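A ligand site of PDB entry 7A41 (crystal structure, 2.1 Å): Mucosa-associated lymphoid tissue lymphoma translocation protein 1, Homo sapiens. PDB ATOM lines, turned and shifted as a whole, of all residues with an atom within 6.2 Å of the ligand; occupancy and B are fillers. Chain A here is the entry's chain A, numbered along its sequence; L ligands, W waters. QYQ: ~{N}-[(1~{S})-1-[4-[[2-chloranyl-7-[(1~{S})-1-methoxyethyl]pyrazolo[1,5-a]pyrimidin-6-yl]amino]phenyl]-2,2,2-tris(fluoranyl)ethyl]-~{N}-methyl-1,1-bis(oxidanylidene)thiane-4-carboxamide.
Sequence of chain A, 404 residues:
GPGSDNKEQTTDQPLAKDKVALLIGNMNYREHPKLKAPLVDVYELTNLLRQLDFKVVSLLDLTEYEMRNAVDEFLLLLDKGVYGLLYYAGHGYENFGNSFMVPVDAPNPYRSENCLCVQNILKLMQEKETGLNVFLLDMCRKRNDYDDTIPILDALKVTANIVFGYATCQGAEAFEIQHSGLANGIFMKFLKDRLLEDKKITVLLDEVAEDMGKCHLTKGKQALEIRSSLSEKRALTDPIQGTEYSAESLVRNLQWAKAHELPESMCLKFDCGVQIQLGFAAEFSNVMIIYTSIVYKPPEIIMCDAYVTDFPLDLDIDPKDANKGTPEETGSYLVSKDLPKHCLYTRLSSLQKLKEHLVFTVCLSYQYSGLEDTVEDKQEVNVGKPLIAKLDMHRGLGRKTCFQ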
ATOM      1  N   LYS A  19      -2.696 -35.442  29.140  1.00  0.00           N
ATOM      2  CA  LYS A  19      -2.114 -34.963  30.375  1.00  0.00           C
ATOM      3  C   LYS A  19      -0.855 -34.204  30.034  1.00  0.00           C
ATOM      4  O   LYS A  19       0.114 -34.802  29.595  1.00  0.00           O
ATOM      5  CB  LYS A  19      -1.778 -36.138  31.301  1.00  0.00           C
ATOM      6  CG  LYS A  19      -3.012 -36.755  31.919  1.00  0.00           C
ATOM      7  CD  LYS A  19      -2.636 -38.018  32.647  1.00  0.00           C
ATOM      8  CE  LYS A  19      -3.677 -38.416  33.634  1.00  0.00           C
ATOM      9  NZ  LYS A  19      -3.199 -39.546  34.458  1.00  0.00           N
ATOM     10  N   VAL A  20      -0.878 -32.876  30.174  1.00  0.00           N
ATOM     11  CA  VAL A  20       0.264 -32.045  29.846  1.00  0.00           C
ATOM     12  C   VAL A  20       0.728 -31.213  31.079  1.00  0.00           C
ATOM     13  O   VAL A  20      -0.095 -30.726  31.860  1.00  0.00           O
ATOM     14  CB  VAL A  20      -0.002 -31.152  28.598  1.00  0.00           C
ATOM     15  CG1 VAL A  20      -0.182 -32.007  27.345  1.00  0.00           C
ATOM     16  CG2 VAL A  20      -1.231 -30.264  28.807  1.00  0.00           C
ATOM     17  N   ALA A  21       2.038 -31.077  31.248  1.00  0.00           N
ATOM     18  CA  ALA A  21       2.585 -30.363  32.372  1.00  0.00           C
ATOM     19  C   ALA A  21       3.747 -29.478  31.963  1.00  0.00           C
ATOM     20  O   ALA A  21       4.604 -29.936  31.203  1.00  0.00           O
ATOM     21  CB  ALA A  21       3.019 -31.345  33.458  1.00  0.00           C
ATOM     22  N   LEU A  22       3.740 -28.208  32.415  1.00  0.00           N
ATOM     23  CA  LEU A  22       4.840 -27.253  32.214  1.00  0.00           C
ATOM     24  C   LEU A  22       5.377 -26.915  33.601  1.00  0.00           C
ATOM     25  O   LEU A  22       4.604 -26.479  34.492  1.00  0.00           O
ATOM     26  CB  LEU A  22       4.395 -25.978  31.483  1.00  0.00           C
ATOM     27  CG  LEU A  22       5.442 -24.862  31.420  1.00  0.00           C
ATOM     28  CD1 LEU A  22       6.703 -25.321  30.678  1.00  0.00           C
ATOM     29  CD2 LEU A  22       4.870 -23.612  30.811  1.00  0.00           C
ATOM     30  N   LYS A  55       2.729 -35.794  29.865  1.00  0.00           N
ATOM     31  CA  LYS A  55       3.776 -35.375  28.956  1.00  0.00           C
ATOM     32  C   LYS A  55       4.263 -34.100  29.671  1.00  0.00           C
ATOM     33  O   LYS A  55       3.460 -33.182  29.936  1.00  0.00           O
ATOM     34  CB  LYS A  55       3.205 -34.988  27.588  1.00  0.00           C
ATOM     35  CG  LYS A  55       2.592 -36.141  26.784  1.00  0.00           C
ATOM     36  CD  LYS A  55       1.922 -35.570  25.502  1.00  0.00           C
ATOM     37  CE  LYS A  55       1.157 -36.587  24.701  1.00  0.00           C
ATOM     38  NZ  LYS A  55       0.274 -37.439  25.559  1.00  0.00           N
ATOM     39  N   VAL A  56       5.546 -34.029  30.020  1.00  0.00           N
ATOM     40  CA  VAL A  56       6.105 -32.924  30.791  1.00  0.00           C
ATOM     41  C   VAL A  56       7.195 -32.159  30.053  1.00  0.00           C
ATOM     42  O   VAL A  56       8.057 -32.754  29.406  1.00  0.00           O
ATOM     43  CB  VAL A  56       6.650 -33.486  32.140  1.00  0.00           C
ATOM     44  CG1 VAL A  56       7.203 -32.379  33.057  1.00  0.00           C
ATOM     45  CG2 VAL A  56       5.575 -34.297  32.871  1.00  0.00           C
ATOM     46  N   VAL A  57       7.185 -30.826  30.190  1.00  0.00           N
ATOM     47  CA  VAL A  57       8.262 -29.971  29.720  1.00  0.00           C
ATOM     48  C   VAL A  57       8.783 -29.300  30.995  1.00  0.00           C
ATOM     49  O   VAL A  57       8.011 -28.678  31.719  1.00  0.00           O
ATOM     50  CB  VAL A  57       7.836 -28.982  28.614  1.00  0.00           C
ATOM     51  CG1 VAL A  57       8.809 -27.795  28.523  1.00  0.00           C
ATOM     52  CG2 VAL A  57       7.740 -29.695  27.265  1.00  0.00           C
ATOM     53  N   LEU A  59      11.729 -26.755  32.565  1.00  0.00           N
ATOM     54  CA  LEU A  59      12.674 -25.723  32.196  1.00  0.00           C
ATOM     55  C   LEU A  59      13.276 -24.989  33.371  1.00  0.00           C
ATOM     56  O   LEU A  59      12.564 -24.571  34.285  1.00  0.00           O
ATOM     57  CB  LEU A  59      11.941 -24.727  31.285  1.00  0.00           C
ATOM     58  CG  LEU A  59      11.355 -25.336  30.003  1.00  0.00           C
ATOM     59  CD1 LEU A  59      10.327 -24.435  29.387  1.00  0.00           C
ATOM     60  CD2 LEU A  59      12.467 -25.663  28.962  1.00  0.00           C
ATOM     61  N   LEU A  62      14.507 -19.227  33.292  1.00  0.00           N
ATOM     62  CA  LEU A  62      13.937 -18.558  32.136  1.00  0.00           C
ATOM     63  C   LEU A  62      13.809 -17.052  32.310  1.00  0.00           C
ATOM     64  O   LEU A  62      13.410 -16.582  33.380  1.00  0.00           O
ATOM     65  CB  LEU A  62      12.555 -19.135  31.787  1.00  0.00           C
ATOM     66  CG  LEU A  62      12.458 -20.630  31.440  1.00  0.00           C
ATOM     67  CD1 LEU A  62      11.009 -20.958  30.990  1.00  0.00           C
ATOM     68  CD2 LEU A  62      13.482 -21.020  30.368  1.00  0.00           C
ATOM     69  N   TYR A  65      10.781 -13.074  28.519  1.00  0.00           N
ATOM     70  CA  TYR A  65      10.392 -13.432  27.159  1.00  0.00           C
ATOM     71  C   TYR A  65      10.253 -14.967  27.028  1.00  0.00           C
ATOM     72  O   TYR A  65       9.272 -15.440  26.437  1.00  0.00           O
ATOM     73  CB  TYR A  65      11.427 -12.838  26.189  1.00  0.00           C
ATOM     74  CG  TYR A  65      11.356 -13.334  24.776  1.00  0.00           C
ATOM     75  CD1 TYR A  65      10.429 -12.813  23.877  1.00  0.00           C
ATOM     76  CD2 TYR A  65      12.266 -14.266  24.292  1.00  0.00           C
ATOM     77  CE1 TYR A  65      10.368 -13.259  22.566  1.00  0.00           C
ATOM     78  CE2 TYR A  65      12.222 -14.715  22.982  1.00  0.00           C
ATOM     79  CZ  TYR A  65      11.273 -14.211  22.119  1.00  0.00           C
ATOM     80  OH  TYR A  65      11.225 -14.645  20.816  1.00  0.00           O
ATOM     81  N   GLU A  66      11.196 -15.731  27.633  1.00  0.00           N
ATOM     82  CA  GLU A  66      11.155 -17.190  27.590  1.00  0.00           C
ATOM     83  C   GLU A  66       9.942 -17.753  28.356  1.00  0.00           C
ATOM     84  O   GLU A  66       9.270 -18.641  27.835  1.00  0.00           O
ATOM     85  CB  GLU A  66      12.466 -17.799  28.099  1.00  0.00           C
ATOM     86  CG  GLU A  66      13.646 -17.527  27.161  1.00  0.00           C
ATOM     87  CD  GLU A  66      15.027 -17.623  27.800  1.00  0.00           C
ATOM     88  OE1 GLU A  66      15.092 -17.854  29.024  1.00  0.00           O
ATOM     89  OE2 GLU A  66      16.036 -17.461  27.077  1.00  0.00           O
ATOM     90  N   MET A  67       9.662 -17.231  29.586  1.00  0.00           N
ATOM     91  CA  MET A  67       8.522 -17.634  30.409  1.00  0.00           C
ATOM     92  C   MET A  67       7.198 -17.304  29.728  1.00  0.00           C
ATOM     93  O   MET A  67       6.280 -18.107  29.779  1.00  0.00           O
ATOM     94  CB  MET A  67       8.536 -16.949  31.788  1.00  0.00           C
ATOM     95  CG  MET A  67       9.626 -17.385  32.660  1.00  0.00           C
ATOM     96  SD  MET A  67       9.520 -16.733  34.320  1.00  0.00           S
ATOM     97  CE  MET A  67       8.062 -17.561  34.887  1.00  0.00           C
ATOM     98  N   ASN A  69       6.644 -16.987  26.495  1.00  0.00           N
ATOM     99  CA  ASN A  69       6.500 -17.905  25.368  1.00  0.00           C
ATOM    100  C   ASN A  69       6.108 -19.288  25.843  1.00  0.00           C
ATOM    101  O   ASN A  69       5.206 -19.869  25.278  1.00  0.00           O
ATOM    102  CB  ASN A  69       7.762 -17.963  24.529  1.00  0.00           C
ATOM    103  CG  ASN A  69       7.942 -16.745  23.662  1.00  0.00           C
ATOM    104  OD1 ASN A  69       6.992 -16.050  23.327  1.00  0.00           O
ATOM    105  ND2 ASN A  69       9.177 -16.456  23.270  1.00  0.00           N
ATOM    106  N   ALA A  70       6.801 -19.830  26.884  1.00  0.00           N
ATOM    107  CA  ALA A  70       6.514 -21.160  27.445  1.00  0.00           C
ATOM    108  C   ALA A  70       5.090 -21.269  27.957  1.00  0.00           C
ATOM    109  O   ALA A  70       4.425 -22.257  27.634  1.00  0.00           O
ATOM    110  CB  ALA A  70       7.505 -21.496  28.569  1.00  0.00           C
ATOM    111  N   VAL A  71       4.604 -20.261  28.716  1.00  0.00           N
ATOM    112  CA  VAL A  71       3.246 -20.252  29.261  1.00  0.00           C
ATOM    113  C   VAL A  71       2.189 -20.148  28.147  1.00  0.00           C
ATOM    114  O   VAL A  71       1.231 -20.922  28.150  1.00  0.00           O
ATOM    115  CB  VAL A  71       3.078 -19.205  30.397  1.00  0.00           C
ATOM    116  CG1 VAL A  71       1.606 -18.998  30.775  1.00  0.00           C
ATOM    117  CG2 VAL A  71       3.886 -19.615  31.633  1.00  0.00           C
ATOM    118  N   GLU A  73       2.460 -21.116  24.987  1.00  0.00           N
ATOM    119  CA  GLU A  73       2.443 -22.371  24.222  1.00  0.00           C
ATOM    120  C   GLU A  73       1.806 -23.505  25.018  1.00  0.00           C
ATOM    121  O   GLU A  73       1.094 -24.336  24.433  1.00  0.00           O
ATOM    122  CB  GLU A  73       3.852 -22.754  23.771  1.00  0.00           C
ATOM    123  CG  GLU A  73       4.394 -21.827  22.692  1.00  0.00           C
ATOM    124  CD  GLU A  73       3.630 -21.936  21.390  1.00  0.00           C
ATOM    125  OE1 GLU A  73       3.289 -23.071  20.993  1.00  0.00           O
ATOM    126  OE2 GLU A  73       3.383 -20.876  20.765  1.00  0.00           O
ATOM    127  N   PHE A  74       2.016 -23.525  26.348  1.00  0.00           N
ATOM    128  CA  PHE A  74       1.407 -24.513  27.221  1.00  0.00           C
ATOM    129  C   PHE A  74      -0.127 -24.334  27.200  1.00  0.00           C
ATOM    130  O   PHE A  74      -0.860 -25.336  27.143  1.00  0.00           O
ATOM    131  CB  PHE A  74       1.949 -24.391  28.669  1.00  0.00           C
ATOM    132  CG  PHE A  74       1.142 -25.140  29.708  1.00  0.00           C
ATOM    133  CD1 PHE A  74       1.231 -26.521  29.817  1.00  0.00           C
ATOM    134  CD2 PHE A  74       0.244 -24.473  30.520  1.00  0.00           C
ATOM    135  CE1 PHE A  74       0.452 -27.212  30.730  1.00  0.00           C
ATOM    136  CE2 PHE A  74      -0.553 -25.168  31.421  1.00  0.00           C
ATOM    137  CZ  PHE A  74      -0.431 -26.534  31.527  1.00  0.00           C
ATOM    138  N   LEU A  77      -2.178 -25.953  24.415  1.00  0.00           N
ATOM    139  CA  LEU A  77      -2.370 -27.397  24.521  1.00  0.00           C
ATOM    140  C   LEU A  77      -3.664 -27.766  25.259  1.00  0.00           C
ATOM    141  O   LEU A  77      -4.053 -28.931  25.261  1.00  0.00           O
ATOM    142  CB  LEU A  77      -1.213 -28.033  25.309  1.00  0.00           C
ATOM    143  CG  LEU A  77       0.212 -27.824  24.796  1.00  0.00           C
ATOM    144  CD1 LEU A  77       1.205 -28.529  25.685  1.00  0.00           C
ATOM    145  CD2 LEU A  77       0.360 -28.316  23.360  1.00  0.00           C
ATOM    146  N   ARG A 252      -0.390 -31.961  19.906  1.00  0.00           N
ATOM    147  CA  ARG A 252       0.122 -32.028  21.270  1.00  0.00           C
ATOM    148  C   ARG A 252       1.286 -32.988  21.402  1.00  0.00           C
ATOM    149  O   ARG A 252       2.311 -32.631  21.992  1.00  0.00           O
ATOM    150  CB  ARG A 252      -0.990 -32.392  22.273  1.00  0.00           C
ATOM    151  CG  ARG A 252      -2.133 -31.399  22.317  1.00  0.00           C
ATOM    152  CD  ARG A 252      -3.043 -31.639  23.507  1.00  0.00           C
ATOM    153  NE  ARG A 252      -3.645 -32.982  23.487  1.00  0.00           N
ATOM    154  CZ  ARG A 252      -4.831 -33.273  22.966  1.00  0.00           C
ATOM    155  NH1 ARG A 252      -5.293 -34.511  22.999  1.00  0.00           N
ATOM    156  NH2 ARG A 252      -5.583 -32.313  22.439  1.00  0.00           N
ATOM    157  N   GLN A 255       4.692 -31.571  19.410  1.00  0.00           N
ATOM    158  CA  GLN A 255       5.451 -30.547  20.117  1.00  0.00           C
ATOM    159  C   GLN A 255       6.270 -31.110  21.270  1.00  0.00           C
ATOM    160  O   GLN A 255       7.466 -30.868  21.375  1.00  0.00           O
ATOM    161  CB  GLN A 255       4.505 -29.428  20.584  1.00  0.00           C
ATOM    162  CG  GLN A 255       3.744 -28.738  19.444  1.00  0.00           C
ATOM    163  CD  GLN A 255       4.615 -28.253  18.301  1.00  0.00           C
ATOM    164  OE1 GLN A 255       4.270 -28.387  17.119  1.00  0.00           O
ATOM    165  NE2 GLN A 255       5.770 -27.671  18.604  1.00  0.00           N
ATOM    166  N   TRP A 256       5.643 -31.959  22.070  1.00  0.00           N
ATOM    167  CA  TRP A 256       6.295 -32.608  23.184  1.00  0.00           C
ATOM    168  C   TRP A 256       7.426 -33.516  22.713  1.00  0.00           C
ATOM    169  O   TRP A 256       8.493 -33.504  23.323  1.00  0.00           O
ATOM    170  CB  TRP A 256       5.264 -33.347  24.001  1.00  0.00           C
ATOM    171  CG  TRP A 256       5.839 -34.291  24.998  1.00  0.00           C
ATOM    172  CD1 TRP A 256       6.414 -33.991  26.191  1.00  0.00           C
ATOM    173  CD2 TRP A 256       5.812 -35.718  24.911  1.00  0.00           C
ATOM    174  NE1 TRP A 256       6.754 -35.140  26.863  1.00  0.00           N
ATOM    175  CE2 TRP A 256       6.394 -36.217  26.089  1.00  0.00           C
ATOM    176  CE3 TRP A 256       5.363 -36.622  23.942  1.00  0.00           C
ATOM    177  CZ2 TRP A 256       6.520 -37.589  26.338  1.00  0.00           C
ATOM    178  CZ3 TRP A 256       5.481 -37.978  24.182  1.00  0.00           C
ATOM    179  CH2 TRP A 256       6.063 -38.448  25.368  1.00  0.00           C
ATOM    180  N   ALA A 259      10.599 -31.501  21.772  1.00  0.00           N
ATOM    181  CA  ALA A 259      11.246 -31.048  23.011  1.00  0.00           C
ATOM    182  C   ALA A 259      12.006 -32.137  23.753  1.00  0.00           C
ATOM    183  O   ALA A 259      12.757 -31.842  24.676  1.00  0.00           O
ATOM    184  CB  ALA A 259      10.205 -30.433  23.936  1.00  0.00           C
ATOM    185  N   ASN A 286      15.734 -27.993  28.902  1.00  0.00           N
ATOM    186  CA  ASN A 286      16.709 -27.033  28.377  1.00  0.00           C
ATOM    187  C   ASN A 286      18.130 -27.259  28.901  1.00  0.00           C
ATOM    188  O   ASN A 286      18.946 -26.345  28.831  1.00  0.00           O
ATOM    189  CB  ASN A 286      16.249 -25.595  28.611  1.00  0.00           C
ATOM    190  CG  ASN A 286      16.141 -25.203  30.079  1.00  0.00           C
ATOM    191  OD1 ASN A 286      15.977 -26.028  31.001  1.00  0.00           O
ATOM    192  ND2 ASN A 286      16.216 -23.921  30.315  1.00  0.00           N
ATOM    193  N   GLN A 352      17.338 -23.214  25.288  1.00  0.00           N
ATOM    194  CA  GLN A 352      16.300 -22.346  24.734  1.00  0.00           C
ATOM    195  C   GLN A 352      16.908 -21.097  24.012  1.00  0.00           C
ATOM    196  O   GLN A 352      16.267 -20.520  23.145  1.00  0.00           O
ATOM    197  CB  GLN A 352      15.250 -21.965  25.814  1.00  0.00           C
ATOM    198  CG  GLN A 352      15.660 -20.902  26.856  1.00  0.00           C
ATOM    199  CD  GLN A 352      16.574 -21.340  27.962  1.00  0.00           C
ATOM    200  OE1 GLN A 352      17.080 -22.453  27.994  1.00  0.00           O
ATOM    201  NE2 GLN A 352      16.843 -20.489  28.916  1.00  0.00           N
ATOM    202  N   LYS A 353      18.164 -20.742  24.310  1.00  0.00           N
ATOM    203  CA  LYS A 353      18.830 -19.604  23.675  1.00  0.00           C
ATOM    204  C   LYS A 353      19.528 -19.952  22.334  1.00  0.00           C
ATOM    205  O   LYS A 353      19.974 -19.069  21.632  1.00  0.00           O
ATOM    206  CB  LYS A 353      19.836 -18.988  24.657  1.00  0.00           C
ATOM    207  CG  LYS A 353      19.175 -18.569  25.978  1.00  0.00           C
ATOM    208  CD  LYS A 353      20.165 -17.815  26.838  1.00  0.00           C
ATOM    209  CE  LYS A 353      19.704 -17.689  28.279  1.00  0.00           C
ATOM    210  NZ  LYS A 353      18.425 -16.937  28.407  1.00  0.00           N
ATOM    211  N   LEU A 354      19.606 -21.227  21.987  1.00  0.00           N
ATOM    212  CA  LEU A 354      20.231 -21.689  20.759  1.00  0.00           C
ATOM    213  C   LEU A 354      19.256 -21.443  19.572  1.00  0.00           C
ATOM    214  O   LEU A 354      18.145 -21.966  19.561  1.00  0.00           O
ATOM    215  CB  LEU A 354      20.507 -23.190  20.927  1.00  0.00           C
ATOM    216  CG  LEU A 354      21.358 -23.908  19.909  1.00  0.00           C
ATOM    217  CD1 LEU A 354      22.771 -23.433  19.955  1.00  0.00           C
ATOM    218  CD2 LEU A 354      21.292 -25.404  20.144  1.00  0.00           C
ATOM    219  N   LYS A 355      19.651 -20.617  18.611  1.00  0.00           N
ATOM    220  CA  LYS A 355      18.823 -20.340  17.430  1.00  0.00           C
ATOM    221  C   LYS A 355      19.343 -21.035  16.156  1.00  0.00           C
ATOM    222  O   LYS A 355      18.625 -21.107  15.149  1.00  0.00           O
ATOM    223  CB  LYS A 355      18.681 -18.820  17.210  1.00  0.00           C
ATOM    224  CG  LYS A 355      18.136 -18.085  18.421  1.00  0.00           C
ATOM    225  CD  LYS A 355      18.703 -16.685  18.533  1.00  0.00           C
ATOM    226  CE  LYS A 355      18.229 -16.027  19.809  1.00  0.00           C
ATOM    227  NZ  LYS A 355      16.743 -16.006  19.886  1.00  0.00           N
ATOM    228  N   ILE A 388      14.469 -28.704  23.910  1.00  0.00           N
ATOM    229  CA  ILE A 388      13.634 -27.525  23.629  1.00  0.00           C
ATOM    230  C   ILE A 388      14.104 -26.673  22.417  1.00  0.00           C
ATOM    231  O   ILE A 388      13.296 -25.941  21.830  1.00  0.00           O
ATOM    232  CB  ILE A 388      13.492 -26.655  24.899  1.00  0.00           C
ATOM    233  CG1 ILE A 388      12.186 -25.863  24.899  1.00  0.00           C
ATOM    234  CG2 ILE A 388      14.711 -25.776  25.130  1.00  0.00           C
ATOM    235  CD1 ILE A 388      10.956 -26.693  25.083  1.00  0.00           C
ATOM    236  N   ALA A 389      15.387 -26.760  22.029  1.00  0.00           N
ATOM    237  CA  ALA A 389      15.889 -26.013  20.870  1.00  0.00           C
ATOM    238  C   ALA A 389      15.308 -26.544  19.541  1.00  0.00           C
ATOM    239  O   ALA A 389      15.384 -25.833  18.544  1.00  0.00           O
ATOM    240  CB  ALA A 389      17.401 -26.010  20.834  1.00  0.00           C
ATOM    241  N   LEU A 391      12.222 -26.827  18.859  1.00  0.00           N
ATOM    242  CA  LEU A 391      11.086 -25.947  18.558  1.00  0.00           C
ATOM    243  C   LEU A 391      11.578 -24.706  17.774  1.00  0.00           C
ATOM    244  O   LEU A 391      12.773 -24.407  17.756  1.00  0.00           O
ATOM    245  CB  LEU A 391      10.450 -25.488  19.879  1.00  0.00           C
ATOM    246  CG  LEU A 391       9.217 -26.222  20.402  1.00  0.00           C
ATOM    247  CD1 LEU A 391       9.422 -27.725  20.452  1.00  0.00           C
ATOM    248  CD2 LEU A 391       8.870 -25.708  21.772  1.00  0.00           C
ATOM    249  N   ASP A 392      10.651 -23.960  17.145  1.00  0.00           N
ATOM    250  CA  ASP A 392      11.014 -22.732  16.417  1.00  0.00           C
ATOM    251  C   ASP A 392       9.894 -21.686  16.445  1.00  0.00           C
ATOM    252  O   ASP A 392       8.833 -21.904  17.048  1.00  0.00           O
ATOM    253  CB  ASP A 392      11.435 -23.051  14.961  1.00  0.00           C
ATOM    254  CG  ASP A 392      12.935 -23.255  14.769  1.00  0.00           C
ATOM    255  OD1 ASP A 392      13.705 -22.884  15.695  1.00  0.00           O
ATOM    256  OD2 ASP A 392      13.330 -23.775  13.703  1.00  0.00           O
HETATM  257  C1  QYQ L   1      10.419 -21.194  25.340  1.00  0.00           C
HETATM  258  C3  QYQ L   1       5.315 -27.208  25.119  1.00  0.00           C
HETATM  259  C11 QYQ L   1       4.124 -28.719  27.994  1.00  0.00           C
HETATM  260  C12 QYQ L   1       5.585 -27.822  23.731  1.00  0.00           C
HETATM  261  C14 QYQ L   1       7.241 -24.204  24.904  1.00  0.00           C
HETATM  262  C15 QYQ L   1       7.415 -23.158  24.007  1.00  0.00           C
HETATM  263  C16 QYQ L   1       8.401 -22.187  24.173  1.00  0.00           C
HETATM  264  C17 QYQ L   1       9.317 -22.273  25.228  1.00  0.00           C
HETATM  265  C18 QYQ L   1       9.167 -23.353  26.110  1.00  0.00           C
HETATM  266  C19 QYQ L   1       8.143 -24.302  25.975  1.00  0.00           C
HETATM  267  C22 QYQ L   1       3.910 -26.600  22.473  1.00  0.00           C
HETATM  268  C23 QYQ L   1       7.065 -28.266  23.648  1.00  0.00           C
HETATM  269  C24 QYQ L   1      11.386 -21.418  26.531  1.00  0.00           C
HETATM  270  C28 QYQ L   1      11.629 -22.209  23.285  1.00  0.00           C
HETATM  271  C29 QYQ L   1      11.316 -19.771  23.521  1.00  0.00           C
HETATM  272  N2  QYQ L   1       4.748 -26.370  27.692  1.00  0.00           N
HETATM  273  C4  QYQ L   1       5.645 -25.942  25.513  1.00  0.00           C
HETATM  274  C5  QYQ L   1       5.258 -25.521  26.891  1.00  0.00           C
HETATM  275  N6  QYQ L   1       6.211 -25.075  24.690  1.00  0.00           N
HETATM  276  C7  QYQ L   1       4.561 -27.706  27.240  1.00  0.00           C
HETATM  277  N8  QYQ L   1       4.791 -28.053  25.985  1.00  0.00           N
HETATM  278  N9  QYQ L   1       4.537 -29.373  25.898  1.00  0.00           N
HETATM  279  C10 QYQ L   1       4.139 -29.787  27.011  1.00  0.00           C
HETATM  280 CL1  QYQ L   1       3.693 -31.406  27.366  1.00  0.00          CL
HETATM  281  N20 QYQ L   1      11.085 -21.032  24.038  1.00  0.00           N
HETATM  282  O21 QYQ L   1       5.313 -26.883  22.661  1.00  0.00           O
HETATM  283  F25 QYQ L   1      12.301 -20.436  26.489  1.00  0.00           F
HETATM  284  F26 QYQ L   1      10.792 -21.335  27.750  1.00  0.00           F
HETATM  285  F27 QYQ L   1      12.107 -22.571  26.467  1.00  0.00           F
HETATM  286  O30 QYQ L   1      10.932 -18.740  24.063  1.00  0.00           O
HETATM  287  C31 QYQ L   1      12.034 -19.525  22.183  1.00  0.00           C
HETATM  288  C32 QYQ L   1      11.224 -18.769  21.097  1.00  0.00           C
HETATM  289  C33 QYQ L   1      11.949 -18.755  19.723  1.00  0.00           C
HETATM  290  S34 QYQ L   1      13.595 -18.026  19.909  1.00  0.00           S
HETATM  291  C35 QYQ L   1      14.313 -19.160  21.108  1.00  0.00           C
HETATM  292  C36 QYQ L   1      13.489 -19.027  22.410  1.00  0.00           C
HETATM  293  O37 QYQ L   1      14.357 -18.097  18.664  1.00  0.00           O
HETATM  294  O38 QYQ L   1      13.467 -16.746  20.585  1.00  0.00           O
HETATM  295  O   HOH W   1       1.314 -24.852  21.750  1.00  0.00           O
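ND2 of Asn 69 sits close to O of Tyr 65 (3.3 Å).
OE1 of Glu 66 sits at hydrogen-bond distance from NE2 of Gln 352.
The side-chain carboxylate of Glu 66 lies within salt-bridge range of the side-chain amino group of Lys 353 (2.8 Å).
The backbone NH of Ala 21 sits at hydrogen-bond distance from the backbone carbonyl oxygen of Lys 55, at 2.9 Å.
O of Lys 19 sits at hydrogen-bond distance from N of Lys 55 (2.8 Å).
The side-chain amide nitrogen (ND2) of Asn 286 lies within hydrogen-bond range of the side-chain amide oxygen (OE1) of Gln 352 (2.9 Å).
N of Val 57 is in hydrogen-bond range of O of Ala 21 (2.9 Å).
ND2 of Asn 69 is in hydrogen-bond range of O30 of the ligand.
OH of Tyr 65 is in hydrogen-bond range of O38 of the ligand (3.1 Å).
An oxygen (O37) of the ligand lies within hydrogen-bond range of the side-chain amino group (NZ) of Lys 355 (3.4 Å).
The backbone carbonyl oxygen (O) of Glu 66 sits close to a fluorine (F26) of the ligand (3.1 Å).
Val 20 touches the ligand (CB to CL1, 3.9 Å).
Ala 21 touches the ligand (O to C11, 3.5 Å).
CD1 of Leu 22 touches N2 of the ligand (3.7 Å).
Lys 55 touches the ligand (O to CL1, 3.1 Å).
CG2 of Val 57 touches N9 of the ligand, at 3.5 Å.
CD1 of Leu 59 touches F26 of the ligand, 3.5 Å away.
CD1 of Leu 62 touches F26 of the ligand (3.3 Å).
Ala 70 touches the ligand (CB to F26, 3.4 Å).
CB of Glu 73 touches N6 of the ligand, 3.4 Å away.
Phe 74 touches the ligand.
Leu 77 touches the ligand (CD1 to N9, 3.4 Å).
Gln 255 touches the ligand (CB to O21, 3.4 Å).
CD1 of Trp 256 touches CL1 of the ligand, 3.9 Å away.
Ala 259 touches the ligand.
Gln 352 touches the ligand (O to C35, 3.1 Å).
CG1 of Ile 388 touches F27 of the ligand, 3.6 Å away.
CD2 of Leu 391 touches C23 of the ligand, 3.6 Å away.
Hydrophobic or aromatic side chains that line the ligand: Val 20, Leu 22, Val 57, Leu 59, Leu 62, Tyr 65, Ala 70, Phe 74, Leu 77, Trp 256, Ala 259, Ile 388 and Leu 391.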
